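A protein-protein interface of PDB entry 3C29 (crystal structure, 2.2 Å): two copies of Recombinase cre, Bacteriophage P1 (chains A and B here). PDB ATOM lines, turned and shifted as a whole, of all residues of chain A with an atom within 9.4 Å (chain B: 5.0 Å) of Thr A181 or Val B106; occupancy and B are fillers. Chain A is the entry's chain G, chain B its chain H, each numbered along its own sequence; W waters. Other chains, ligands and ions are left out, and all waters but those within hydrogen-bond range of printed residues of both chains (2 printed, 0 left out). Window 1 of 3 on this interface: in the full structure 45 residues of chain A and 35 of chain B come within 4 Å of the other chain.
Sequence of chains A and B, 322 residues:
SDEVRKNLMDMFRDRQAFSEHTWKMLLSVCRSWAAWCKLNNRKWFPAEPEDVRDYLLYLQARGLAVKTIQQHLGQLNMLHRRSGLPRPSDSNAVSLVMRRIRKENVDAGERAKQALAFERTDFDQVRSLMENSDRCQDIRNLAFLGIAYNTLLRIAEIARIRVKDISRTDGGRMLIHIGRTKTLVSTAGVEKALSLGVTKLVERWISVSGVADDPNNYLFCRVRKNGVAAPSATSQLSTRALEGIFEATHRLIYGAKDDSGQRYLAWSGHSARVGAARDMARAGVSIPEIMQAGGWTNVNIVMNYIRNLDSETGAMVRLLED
NH2 of Arg B111 lies within hydrogen-bond range of O of Ile A178 (3.0 Å). The guanidinium group (NH2) of Arg B111 sits at hydrogen-bond distance from the backbone carbonyl oxygen (O) of Gly A179, at 2.9 Å. The guanidinium group of Arg A180 is in salt-bridge range of the side-chain carboxylate of Asp B107 (3.4 Å).
NH2 of Arg A160 sits at hydrogen-bond distance from O of Arg A180, at 3.3 Å. ND1 of His A177 sits at hydrogen-bond distance from O of Val A190, 3.2 Å away. The backbone carbonyl oxygen (O) of Val A190 sits at hydrogen-bond distance from the backbone NH (N) of Ile A178 (2.8 Å). The side-chain hydroxyl of Thr A181 is in hydrogen-bond range of the backbone carbonyl oxygen of Thr A183. O of Asn B105 lies within hydrogen-bond range of N of Glu B110 (2.8 Å). The backbone carbonyl oxygen (O) of Gly B109 lies within hydrogen-bond range of the guanidinium group (NE) of Arg B111, 2.8 Å away.
Among the printed residues, merely in contact across the chains: His A177 with Arg B111, Gly A179 with Gly B109, Arg A180 with Val B106, Thr A181 with Val B106, Thr A181 with Glu B110, Thr A181 with Arg B111, Leu A184 with Val B106, Leu A184 with Glu B110, Leu A184 with Arg B111 and Val A190 with Arg B111.
Of chain B, only Val B106 (3.6 Å), Glu B110 (3.6 Å) and Arg B111 (3.6 Å) come within 4 Å of Thr A181. Of chain A, only Arg A180 (3.7 Å), Thr A181 (3.6 Å) and Leu A184 (3.8 Å) come within 4 Å of Val B106. Ala B108 touches none of the printed residues of chain A. Of the printed residues of chain B, Val A190 touches Arg B111 (3.7 Å). Of the printed residues of chain B, His A177 touches Arg B111 (3.6 Å). Of the printed residues of chain B, Arg A180 touches Val B106 (3.7 Å) and Asp B107 (3.4 Å). Arg B102 touches none of the printed residues of chain A. The nearest printed residue of chain B that does not touch Thr A181 is Gly B109 (5.5 Å). The nearest residue of chain A that does not touch Val B106 is Thr A183 (4.2 Å).
Of the 11 printed residues of chain B, 5 touch a printed residue of chain A. Printed residues of chain B that touch a printed residue of chain A: Val B106, Asp B107, Gly B109, Glu B110 and Arg B111. Of the 22 printed residues of chain A, 7 touch a printed residue of chain B. Hydrophobic or aromatic side chains of chain A within 4 Å of the printed part of chain B: His A177, Leu A184 and Val A190. Among the printed residues, Asp or Glu carboxylates within 4 Å of a Lys or Arg side-chain nitrogen of the other chain: Arg A180 with Asp B107 (3.4 Å).
No position is printed for both chains.
Water W1 lies within hydrogen-bond range of O of Val B106 (2.6 Å), O of Glu B110 (2.8 Å), N of Thr A181 (2.8 Å) and NH2 of Arg B111 (3.5 Å). Water W2 bridges the backbone NH (N) of Leu A184 and the guanidinium group (NE) of Arg B102.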
ATOM      1  N   LEU A 153     -13.396  -7.973   1.389  1.00  0.00           N
ATOM      2  CA  LEU A 153     -14.256  -7.027   2.079  1.00  0.00           C
ATOM      3  C   LEU A 153     -13.660  -5.620   2.033  1.00  0.00           C
ATOM      4  O   LEU A 153     -12.432  -5.446   2.029  1.00  0.00           O
ATOM      5  CB  LEU A 153     -14.541  -7.477   3.527  1.00  0.00           C
ATOM      6  CG  LEU A 153     -15.451  -8.709   3.723  1.00  0.00           C
ATOM      7  CD1 LEU A 153     -15.407  -9.159   5.176  1.00  0.00           C
ATOM      8  CD2 LEU A 153     -16.896  -8.465   3.260  1.00  0.00           C
ATOM      9  N   ARG A 154     -14.537  -4.622   1.950  1.00  0.00           N
ATOM     10  CA  ARG A 154     -14.126  -3.217   1.976  1.00  0.00           C
ATOM     11  C   ARG A 154     -13.713  -2.840   3.397  1.00  0.00           C
ATOM     12  O   ARG A 154     -14.154  -3.469   4.360  1.00  0.00           O
ATOM     13  CB  ARG A 154     -15.272  -2.315   1.483  1.00  0.00           C
ATOM     14  CG  ARG A 154     -15.673  -2.593   0.011  1.00  0.00           C
ATOM     15  CD  ARG A 154     -17.040  -1.999  -0.342  1.00  0.00           C
ATOM     16  NE  ARG A 154     -17.535  -2.568  -1.602  1.00  0.00           N
ATOM     17  CZ  ARG A 154     -18.557  -3.414  -1.705  1.00  0.00           C
ATOM     18  NH1 ARG A 154     -19.245  -3.786  -0.616  1.00  0.00           N
ATOM     19  NH2 ARG A 154     -18.905  -3.878  -2.912  1.00  0.00           N
ATOM     20  N   ALA A 156     -14.633  -0.608   5.502  1.00  0.00           N
ATOM     21  CA  ALA A 156     -15.725  -0.337   6.449  1.00  0.00           C
ATOM     22  C   ALA A 156     -16.393  -1.638   6.904  1.00  0.00           C
ATOM     23  O   ALA A 156     -16.838  -1.744   8.045  1.00  0.00           O
ATOM     24  CB  ALA A 156     -16.780   0.679   5.870  1.00  0.00           C
ATOM     25  N   GLU A 157     -16.429  -2.625   6.021  1.00  0.00           N
ATOM     26  CA  GLU A 157     -17.018  -3.929   6.347  1.00  0.00           C
ATOM     27  C   GLU A 157     -16.115  -4.718   7.301  1.00  0.00           C
ATOM     28  O   GLU A 157     -16.598  -5.382   8.231  1.00  0.00           O
ATOM     29  CB  GLU A 157     -17.319  -4.722   5.064  1.00  0.00           C
ATOM     30  CG  GLU A 157     -18.245  -3.967   4.119  1.00  0.00           C
ATOM     31  CD  GLU A 157     -18.414  -4.578   2.695  1.00  0.00           C
ATOM     32  OE1 GLU A 157     -19.497  -4.316   2.109  1.00  0.00           O
ATOM     33  OE2 GLU A 157     -17.498  -5.268   2.145  1.00  0.00           O
ATOM     34  N   ARG A 160     -16.287  -3.437  10.995  1.00  0.00           N
ATOM     35  CA  ARG A 160     -17.544  -3.837  11.617  1.00  0.00           C
ATOM     36  C   ARG A 160     -17.588  -5.300  12.030  1.00  0.00           C
ATOM     37  O   ARG A 160     -18.563  -5.715  12.637  1.00  0.00           O
ATOM     38  CB  ARG A 160     -18.705  -3.714  10.607  1.00  0.00           C
ATOM     39  CG  ARG A 160     -19.190  -2.345  10.353  1.00  0.00           C
ATOM     40  CD  ARG A 160     -20.619  -2.325   9.787  1.00  0.00           C
ATOM     41  NE  ARG A 160     -20.787  -3.037   8.524  1.00  0.00           N
ATOM     42  CZ  ARG A 160     -20.677  -2.482   7.317  1.00  0.00           C
ATOM     43  NH1 ARG A 160     -20.367  -1.208   7.182  1.00  0.00           N
ATOM     44  NH2 ARG A 160     -20.889  -3.214   6.243  1.00  0.00           N
ATOM     45  N   ILE A 176     -16.582 -16.146   8.379  1.00  0.00           N
ATOM     46  CA  ILE A 176     -17.045 -14.850   8.864  1.00  0.00           C
ATOM     47  C   ILE A 176     -18.428 -14.541   8.284  1.00  0.00           C
ATOM     48  O   ILE A 176     -18.579 -14.321   7.078  1.00  0.00           O
ATOM     49  CB  ILE A 176     -16.066 -13.678   8.497  1.00  0.00           C
ATOM     50  CG1 ILE A 176     -14.614 -13.976   8.957  1.00  0.00           C
ATOM     51  CG2 ILE A 176     -16.594 -12.338   9.057  1.00  0.00           C
ATOM     52  CD1 ILE A 176     -13.554 -12.987   8.400  1.00  0.00           C
ATOM     53  N   HIS A 177     -19.431 -14.547   9.156  1.00  0.00           N
ATOM     54  CA  HIS A 177     -20.755 -14.129   8.776  1.00  0.00           C
ATOM     55  C   HIS A 177     -20.751 -12.610   8.613  1.00  0.00           C
ATOM     56  O   HIS A 177     -20.125 -11.895   9.396  1.00  0.00           O
ATOM     57  CB  HIS A 177     -21.773 -14.575   9.826  1.00  0.00           C
ATOM     58  CG  HIS A 177     -23.174 -14.131   9.529  1.00  0.00           C
ATOM     59  ND1 HIS A 177     -23.980 -14.781   8.616  1.00  0.00           N
ATOM     60  CD2 HIS A 177     -23.907 -13.101  10.019  1.00  0.00           C
ATOM     61  CE1 HIS A 177     -25.153 -14.174   8.563  1.00  0.00           C
ATOM     62  NE2 HIS A 177     -25.136 -13.155   9.407  1.00  0.00           N
ATOM     63  N   ILE A 178     -21.416 -12.132   7.570  1.00  0.00           N
ATOM     64  CA  ILE A 178     -21.524 -10.708   7.289  1.00  0.00           C
ATOM     65  C   ILE A 178     -22.714 -10.154   8.071  1.00  0.00           C
ATOM     66  O   ILE A 178     -23.869 -10.402   7.717  1.00  0.00           O
ATOM     67  CB  ILE A 178     -21.641 -10.431   5.753  1.00  0.00           C
ATOM     68  CG1 ILE A 178     -20.344 -10.869   5.037  1.00  0.00           C
ATOM     69  CG2 ILE A 178     -21.903  -8.944   5.468  1.00  0.00           C
ATOM     70  CD1 ILE A 178     -20.484 -11.054   3.500  1.00  0.00           C
ATOM     71  N   GLY A 179     -22.426  -9.408   9.136  1.00  0.00           N
ATOM     72  CA  GLY A 179     -23.473  -8.948  10.065  1.00  0.00           C
ATOM     73  C   GLY A 179     -24.371  -7.917   9.408  1.00  0.00           C
ATOM     74  O   GLY A 179     -25.581  -7.965   9.552  1.00  0.00           O
ATOM     75  N   ARG A 180     -23.763  -6.975   8.693  1.00  0.00           N
ATOM     76  CA  ARG A 180     -24.496  -5.981   7.938  1.00  0.00           C
ATOM     77  C   ARG A 180     -24.033  -6.052   6.495  1.00  0.00           C
ATOM     78  O   ARG A 180     -22.862  -5.815   6.192  1.00  0.00           O
ATOM     79  CB  ARG A 180     -24.275  -4.580   8.505  1.00  0.00           C
ATOM     80  CG  ARG A 180     -24.747  -3.446   7.552  1.00  0.00           C
ATOM     81  CD  ARG A 180     -24.431  -2.086   8.150  1.00  0.00           C
ATOM     82  NE  ARG A 180     -24.235  -1.042   7.143  1.00  0.00           N
ATOM     83  CZ  ARG A 180     -23.812   0.203   7.422  1.00  0.00           C
ATOM     84  NH1 ARG A 180     -23.564   0.575   8.689  1.00  0.00           N
ATOM     85  NH2 ARG A 180     -23.639   1.084   6.436  1.00  0.00           N
ATOM     86  N   THR A 181     -24.955  -6.373   5.596  1.00  0.00           N
ATOM     87  CA  THR A 181     -24.615  -6.448   4.181  1.00  0.00           C
ATOM     88  C   THR A 181     -24.502  -5.057   3.564  1.00  0.00           C
ATOM     89  O   THR A 181     -24.955  -4.058   4.149  1.00  0.00           O
ATOM     90  CB  THR A 181     -25.596  -7.359   3.415  1.00  0.00           C
ATOM     91  OG1 THR A 181     -26.951  -6.999   3.740  1.00  0.00           O
ATOM     92  CG2 THR A 181     -25.364  -8.849   3.800  1.00  0.00           C
ATOM     93  N   LYS A 182     -23.889  -4.996   2.380  1.00  0.00           N
ATOM     94  CA  LYS A 182     -23.696  -3.747   1.658  1.00  0.00           C
ATOM     95  C   LYS A 182     -25.033  -3.214   1.148  1.00  0.00           C
ATOM     96  O   LYS A 182     -25.207  -2.001   1.000  1.00  0.00           O
ATOM     97  CB  LYS A 182     -22.749  -3.967   0.466  1.00  0.00           C
ATOM     98  N   THR A 183     -25.934  -4.143   0.811  1.00  0.00           N
ATOM     99  CA  THR A 183     -27.214  -3.856   0.169  1.00  0.00           C
ATOM    100  C   THR A 183     -28.182  -4.953   0.629  1.00  0.00           C
ATOM    101  O   THR A 183     -27.744  -5.925   1.239  1.00  0.00           O
ATOM    102  CB  THR A 183     -27.089  -3.844  -1.394  1.00  0.00           C
ATOM    103  OG1 THR A 183     -26.571  -5.096  -1.852  1.00  0.00           O
ATOM    104  CG2 THR A 183     -26.124  -2.787  -1.869  1.00  0.00           C
ATOM    105  N   LEU A 184     -29.485  -4.776   0.373  1.00  0.00           N
ATOM    106  CA  LEU A 184     -30.508  -5.769   0.701  1.00  0.00           C
ATOM    107  C   LEU A 184     -30.249  -7.132   0.049  1.00  0.00           C
ATOM    108  O   LEU A 184     -30.348  -8.148   0.690  1.00  0.00           O
ATOM    109  CB  LEU A 184     -31.895  -5.267   0.272  1.00  0.00           C
ATOM    110  CG  LEU A 184     -33.077  -6.118   0.780  1.00  0.00           C
ATOM    111  CD1 LEU A 184     -33.172  -6.066   2.327  1.00  0.00           C
ATOM    112  CD2 LEU A 184     -34.373  -5.693   0.141  1.00  0.00           C
ATOM    113  N   VAL A 185     -29.940  -7.128  -1.243  1.00  0.00           N
ATOM    114  CA  VAL A 185     -29.623  -8.350  -1.967  1.00  0.00           C
ATOM    115  C   VAL A 185     -28.110  -8.401  -2.032  1.00  0.00           C
ATOM    116  O   VAL A 185     -27.497  -7.725  -2.840  1.00  0.00           O
ATOM    117  CB  VAL A 185     -30.271  -8.373  -3.376  1.00  0.00           C
ATOM    118  CG1 VAL A 185     -29.962  -9.702  -4.093  1.00  0.00           C
ATOM    119  CG2 VAL A 185     -31.827  -8.168  -3.285  1.00  0.00           C
ATOM    120  N   SER A 186     -27.504  -9.190  -1.155  1.00  0.00           N
ATOM    121  CA  SER A 186     -26.048  -9.139  -0.983  1.00  0.00           C
ATOM    122  C   SER A 186     -25.338  -9.991  -2.032  1.00  0.00           C
ATOM    123  O   SER A 186     -25.258 -11.217  -1.911  1.00  0.00           O
ATOM    124  CB  SER A 186     -25.675  -9.612   0.416  1.00  0.00           C
ATOM    125  OG  SER A 186     -24.284  -9.576   0.592  1.00  0.00           O
ATOM    126  N   THR A 187     -24.838  -9.324  -3.059  1.00  0.00           N
ATOM    127  CA  THR A 187     -24.139  -9.985  -4.161  1.00  0.00           C
ATOM    128  C   THR A 187     -22.896 -10.743  -3.715  1.00  0.00           C
ATOM    129  O   THR A 187     -22.499 -11.740  -4.341  1.00  0.00           O
ATOM    130  CB  THR A 187     -23.765  -8.943  -5.237  1.00  0.00           C
ATOM    131  OG1 THR A 187     -24.983  -8.349  -5.702  1.00  0.00           O
ATOM    132  CG2 THR A 187     -23.059  -9.612  -6.445  1.00  0.00           C
ATOM    133  N   ALA A 188     -22.260 -10.265  -2.649  1.00  0.00           N
ATOM    134  CA  ALA A 188     -21.075 -10.957  -2.157  1.00  0.00           C
ATOM    135  C   ALA A 188     -21.463 -12.106  -1.239  1.00  0.00           C
ATOM    136  O   ALA A 188     -20.592 -12.806  -0.748  1.00  0.00           O
ATOM    137  CB  ALA A 188     -20.106  -9.973  -1.448  1.00  0.00           C
ATOM    138  N   GLY A 189     -22.765 -12.303  -1.007  1.00  0.00           N
ATOM    139  CA  GLY A 189     -23.228 -13.375  -0.112  1.00  0.00           C
ATOM    140  C   GLY A 189     -23.364 -12.910   1.336  1.00  0.00           C
ATOM    141  O   GLY A 189     -23.355 -11.698   1.608  1.00  0.00           O
ATOM    142  N   VAL A 190     -23.468 -13.870   2.261  1.00  0.00           N
ATOM    143  CA  VAL A 190     -23.754 -13.568   3.661  1.00  0.00           C
ATOM    144  C   VAL A 190     -22.610 -14.034   4.577  1.00  0.00           C
ATOM    145  O   VAL A 190     -22.694 -13.917   5.798  1.00  0.00           O
ATOM    146  CB  VAL A 190     -25.124 -14.203   4.142  1.00  0.00           C
ATOM    147  CG1 VAL A 190     -26.321 -13.673   3.338  1.00  0.00           C
ATOM    148  CG2 VAL A 190     -25.087 -15.752   4.104  1.00  0.00           C
ATOM    149  N   GLU A 191     -21.548 -14.551   3.970  1.00  0.00           N
ATOM    150  CA  GLU A 191     -20.467 -15.246   4.684  1.00  0.00           C
ATOM    151  C   GLU A 191     -19.208 -15.172   3.874  1.00  0.00           C
ATOM    152  O   GLU A 191     -19.275 -15.248   2.648  1.00  0.00           O
ATOM    153  CB  GLU A 191     -20.736 -16.749   4.722  1.00  0.00           C
ATOM    154  CG  GLU A 191     -21.623 -17.243   5.761  1.00  0.00           C
ATOM    155  CD  GLU A 191     -21.889 -18.703   5.521  1.00  0.00           C
ATOM    156  OE1 GLU A 191     -22.619 -19.319   6.330  1.00  0.00           O
ATOM    157  OE2 GLU A 191     -21.348 -19.233   4.522  1.00  0.00           O
ATOM    158  N   LYS A 192     -18.069 -15.140   4.555  1.00  0.00           N
ATOM    159  CA  LYS A 192     -16.763 -15.231   3.899  1.00  0.00           C
ATOM    160  C   LYS A 192     -15.906 -16.271   4.614  1.00  0.00           C
ATOM    161  O   LYS A 192     -15.687 -16.186   5.836  1.00  0.00           O
ATOM    162  CB  LYS A 192     -16.050 -13.879   3.920  1.00  0.00           C
ATOM    163  CG  LYS A 192     -16.728 -12.764   3.158  1.00  0.00           C
ATOM    164  CD  LYS A 192     -16.572 -12.921   1.612  1.00  0.00           C
ATOM    165  CE  LYS A 192     -17.051 -11.663   0.907  1.00  0.00           C
ATOM    166  NZ  LYS A 192     -16.458 -11.546  -0.439  1.00  0.00           N
ATOM    167  N   ILE B 101     -36.398   3.306   5.725  1.00  0.00           N
ATOM    168  CA  ILE B 101     -36.757   1.999   6.268  1.00  0.00           C
ATOM    169  C   ILE B 101     -35.804   0.939   5.725  1.00  0.00           C
ATOM    170  O   ILE B 101     -35.322   0.074   6.462  1.00  0.00           O
ATOM    171  CB  ILE B 101     -38.255   1.654   5.907  1.00  0.00           C
ATOM    172  CG1 ILE B 101     -39.220   2.574   6.695  1.00  0.00           C
ATOM    173  CG2 ILE B 101     -38.547   0.167   6.126  1.00  0.00           C
ATOM    174  CD1 ILE B 101     -40.670   2.507   6.247  1.00  0.00           C
ATOM    175  N   ARG B 102     -35.539   1.003   4.425  1.00  0.00           N
ATOM    176  CA  ARG B 102     -34.636   0.058   3.791  1.00  0.00           C
ATOM    177  C   ARG B 102     -33.250   0.127   4.430  1.00  0.00           C
ATOM    178  O   ARG B 102     -32.684  -0.888   4.814  1.00  0.00           O
ATOM    179  CB  ARG B 102     -34.563   0.368   2.301  1.00  0.00           C
ATOM    180  CG  ARG B 102     -33.690  -0.562   1.456  1.00  0.00           C
ATOM    181  CD  ARG B 102     -33.395   0.097   0.042  1.00  0.00           C
ATOM    182  NE  ARG B 102     -32.041   0.587   0.191  1.00  0.00           N
ATOM    183  CZ  ARG B 102     -31.639   1.853   0.226  1.00  0.00           C
ATOM    184  NH1 ARG B 102     -32.477   2.873   0.008  1.00  0.00           N
ATOM    185  NH2 ARG B 102     -30.344   2.078   0.451  1.00  0.00           N
ATOM    186  N   LYS B 103     -32.735   1.345   4.569  1.00  0.00           N
ATOM    187  CA  LYS B 103     -31.383   1.595   5.066  1.00  0.00           C
ATOM    188  C   LYS B 103     -31.266   1.182   6.536  1.00  0.00           C
ATOM    189  O   LYS B 103     -30.352   0.443   6.913  1.00  0.00           O
ATOM    190  CB  LYS B 103     -31.073   3.083   4.868  1.00  0.00           C
ATOM    191  CG  LYS B 103     -29.639   3.408   4.505  1.00  0.00           C
ATOM    192  CD  LYS B 103     -29.603   4.558   3.500  1.00  0.00           C
ATOM    193  CE  LYS B 103     -28.195   4.827   2.963  1.00  0.00           C
ATOM    194  NZ  LYS B 103     -27.220   3.694   3.027  1.00  0.00           N
ATOM    195  N   GLU B 104     -32.229   1.595   7.361  1.00  0.00           N
ATOM    196  CA  GLU B 104     -32.283   1.154   8.778  1.00  0.00           C
ATOM    197  C   GLU B 104     -32.369  -0.357   8.970  1.00  0.00           C
ATOM    198  O   GLU B 104     -31.664  -0.897   9.776  1.00  0.00           O
ATOM    199  CB  GLU B 104     -33.501   1.767   9.486  1.00  0.00           C
ATOM    200  CG  GLU B 104     -33.364   3.225   9.795  1.00  0.00           C
ATOM    201  CD  GLU B 104     -34.664   3.822  10.314  1.00  0.00           C
ATOM    202  OE1 GLU B 104     -34.623   4.989  10.761  1.00  0.00           O
ATOM    203  OE2 GLU B 104     -35.720   3.132  10.277  1.00  0.00           O
ATOM    204  N   ASN B 105     -33.260  -1.032   8.252  1.00  0.00           N
ATOM    205  CA  ASN B 105     -33.353  -2.496   8.344  1.00  0.00           C
ATOM    206  C   ASN B 105     -32.080  -3.252   7.920  1.00  0.00           C
ATOM    207  O   ASN B 105     -31.666  -4.204   8.573  1.00  0.00           O
ATOM    208  CB  ASN B 105     -34.556  -2.998   7.563  1.00  0.00           C
ATOM    209  CG  ASN B 105     -35.867  -2.753   8.306  1.00  0.00           C
ATOM    210  OD1 ASN B 105     -35.984  -1.814   9.120  1.00  0.00           O
ATOM    211  ND2 ASN B 105     -36.858  -3.591   8.028  1.00  0.00           N
ATOM    212  N   VAL B 106     -31.482  -2.825   6.818  1.00  0.00           N
ATOM    213  CA  VAL B 106     -30.236  -3.433   6.335  1.00  0.00           C
ATOM    214  C   VAL B 106     -29.102  -3.193   7.364  1.00  0.00           C
ATOM    215  O   VAL B 106     -28.344  -4.113   7.702  1.00  0.00           O
ATOM    216  CB  VAL B 106     -29.872  -2.917   4.930  1.00  0.00           C
ATOM    217  CG1 VAL B 106     -28.486  -3.357   4.538  1.00  0.00           C
ATOM    218  CG2 VAL B 106     -30.896  -3.422   3.894  1.00  0.00           C
ATOM    219  N   ASP B 107     -29.026  -1.956   7.868  1.00  0.00           N
ATOM    220  CA  ASP B 107     -28.058  -1.585   8.921  1.00  0.00           C
ATOM    221  C   ASP B 107     -28.242  -2.391  10.204  1.00  0.00           C
ATOM    222  O   ASP B 107     -27.273  -2.679  10.874  1.00  0.00           O
ATOM    223  CB  ASP B 107     -28.089  -0.075   9.190  1.00  0.00           C
ATOM    224  CG  ASP B 107     -27.618   0.770   7.968  1.00  0.00           C
ATOM    225  OD1 ASP B 107     -27.381   0.242   6.841  1.00  0.00           O
ATOM    226  OD2 ASP B 107     -27.516   2.007   8.123  1.00  0.00           O
ATOM    227  N   ALA B 108     -29.481  -2.774  10.519  1.00  0.00           N
ATOM    228  CA  ALA B 108     -29.806  -3.690  11.626  1.00  0.00           C
ATOM    229  C   ALA B 108     -29.600  -5.188  11.267  1.00  0.00           C
ATOM    230  O   ALA B 108     -29.876  -6.066  12.085  1.00  0.00           O
ATOM    231  CB  ALA B 108     -31.265  -3.462  12.120  1.00  0.00           C
ATOM    232  N   GLY B 109     -29.136  -5.490  10.059  1.00  0.00           N
ATOM    233  CA  GLY B 109     -28.770  -6.856   9.735  1.00  0.00           C
ATOM    234  C   GLY B 109     -29.658  -7.540   8.710  1.00  0.00           C
ATOM    235  O   GLY B 109     -29.437  -8.719   8.384  1.00  0.00           O
ATOM    236  N   GLU B 110     -30.662  -6.827   8.180  1.00  0.00           N
ATOM    237  CA  GLU B 110     -31.554  -7.460   7.202  1.00  0.00           C
ATOM    238  C   GLU B 110     -30.865  -7.692   5.862  1.00  0.00           C
ATOM    239  O   GLU B 110     -30.154  -6.830   5.374  1.00  0.00           O
ATOM    240  CB  GLU B 110     -32.846  -6.659   6.974  1.00  0.00           C
ATOM    241  CG  GLU B 110     -33.801  -7.389   5.994  1.00  0.00           C
ATOM    242  CD  GLU B 110     -35.208  -6.825   5.950  1.00  0.00           C
ATOM    243  OE1 GLU B 110     -35.617  -6.135   6.905  1.00  0.00           O
ATOM    244  OE2 GLU B 110     -35.924  -7.109   4.961  1.00  0.00           O
ATOM    245  N   ARG B 111     -31.095  -8.869   5.280  1.00  0.00           N
ATOM    246  CA  ARG B 111     -30.768  -9.138   3.889  1.00  0.00           C
ATOM    247  C   ARG B 111     -31.827 -10.069   3.287  1.00  0.00           C
ATOM    248  O   ARG B 111     -32.431 -10.883   4.012  1.00  0.00           O
ATOM    249  CB  ARG B 111     -29.341  -9.704   3.731  1.00  0.00           C
ATOM    250  CG  ARG B 111     -29.137 -11.209   4.085  1.00  0.00           C
ATOM    251  CD  ARG B 111     -29.217 -11.546   5.601  1.00  0.00           C
ATOM    252  NE  ARG B 111     -28.518 -10.539   6.400  1.00  0.00           N
ATOM    253  CZ  ARG B 111     -27.234 -10.584   6.731  1.00  0.00           C
ATOM    254  NH1 ARG B 111     -26.468 -11.628   6.368  1.00  0.00           N
ATOM    255  NH2 ARG B 111     -26.717  -9.570   7.423  1.00  0.00           N
HETATM  256  O   HOH W   1     -27.623  -6.350   6.487  1.00  0.00           O
HETATM  257  O   HOH W   2     -30.114  -1.941   0.059  1.00  0.00           O
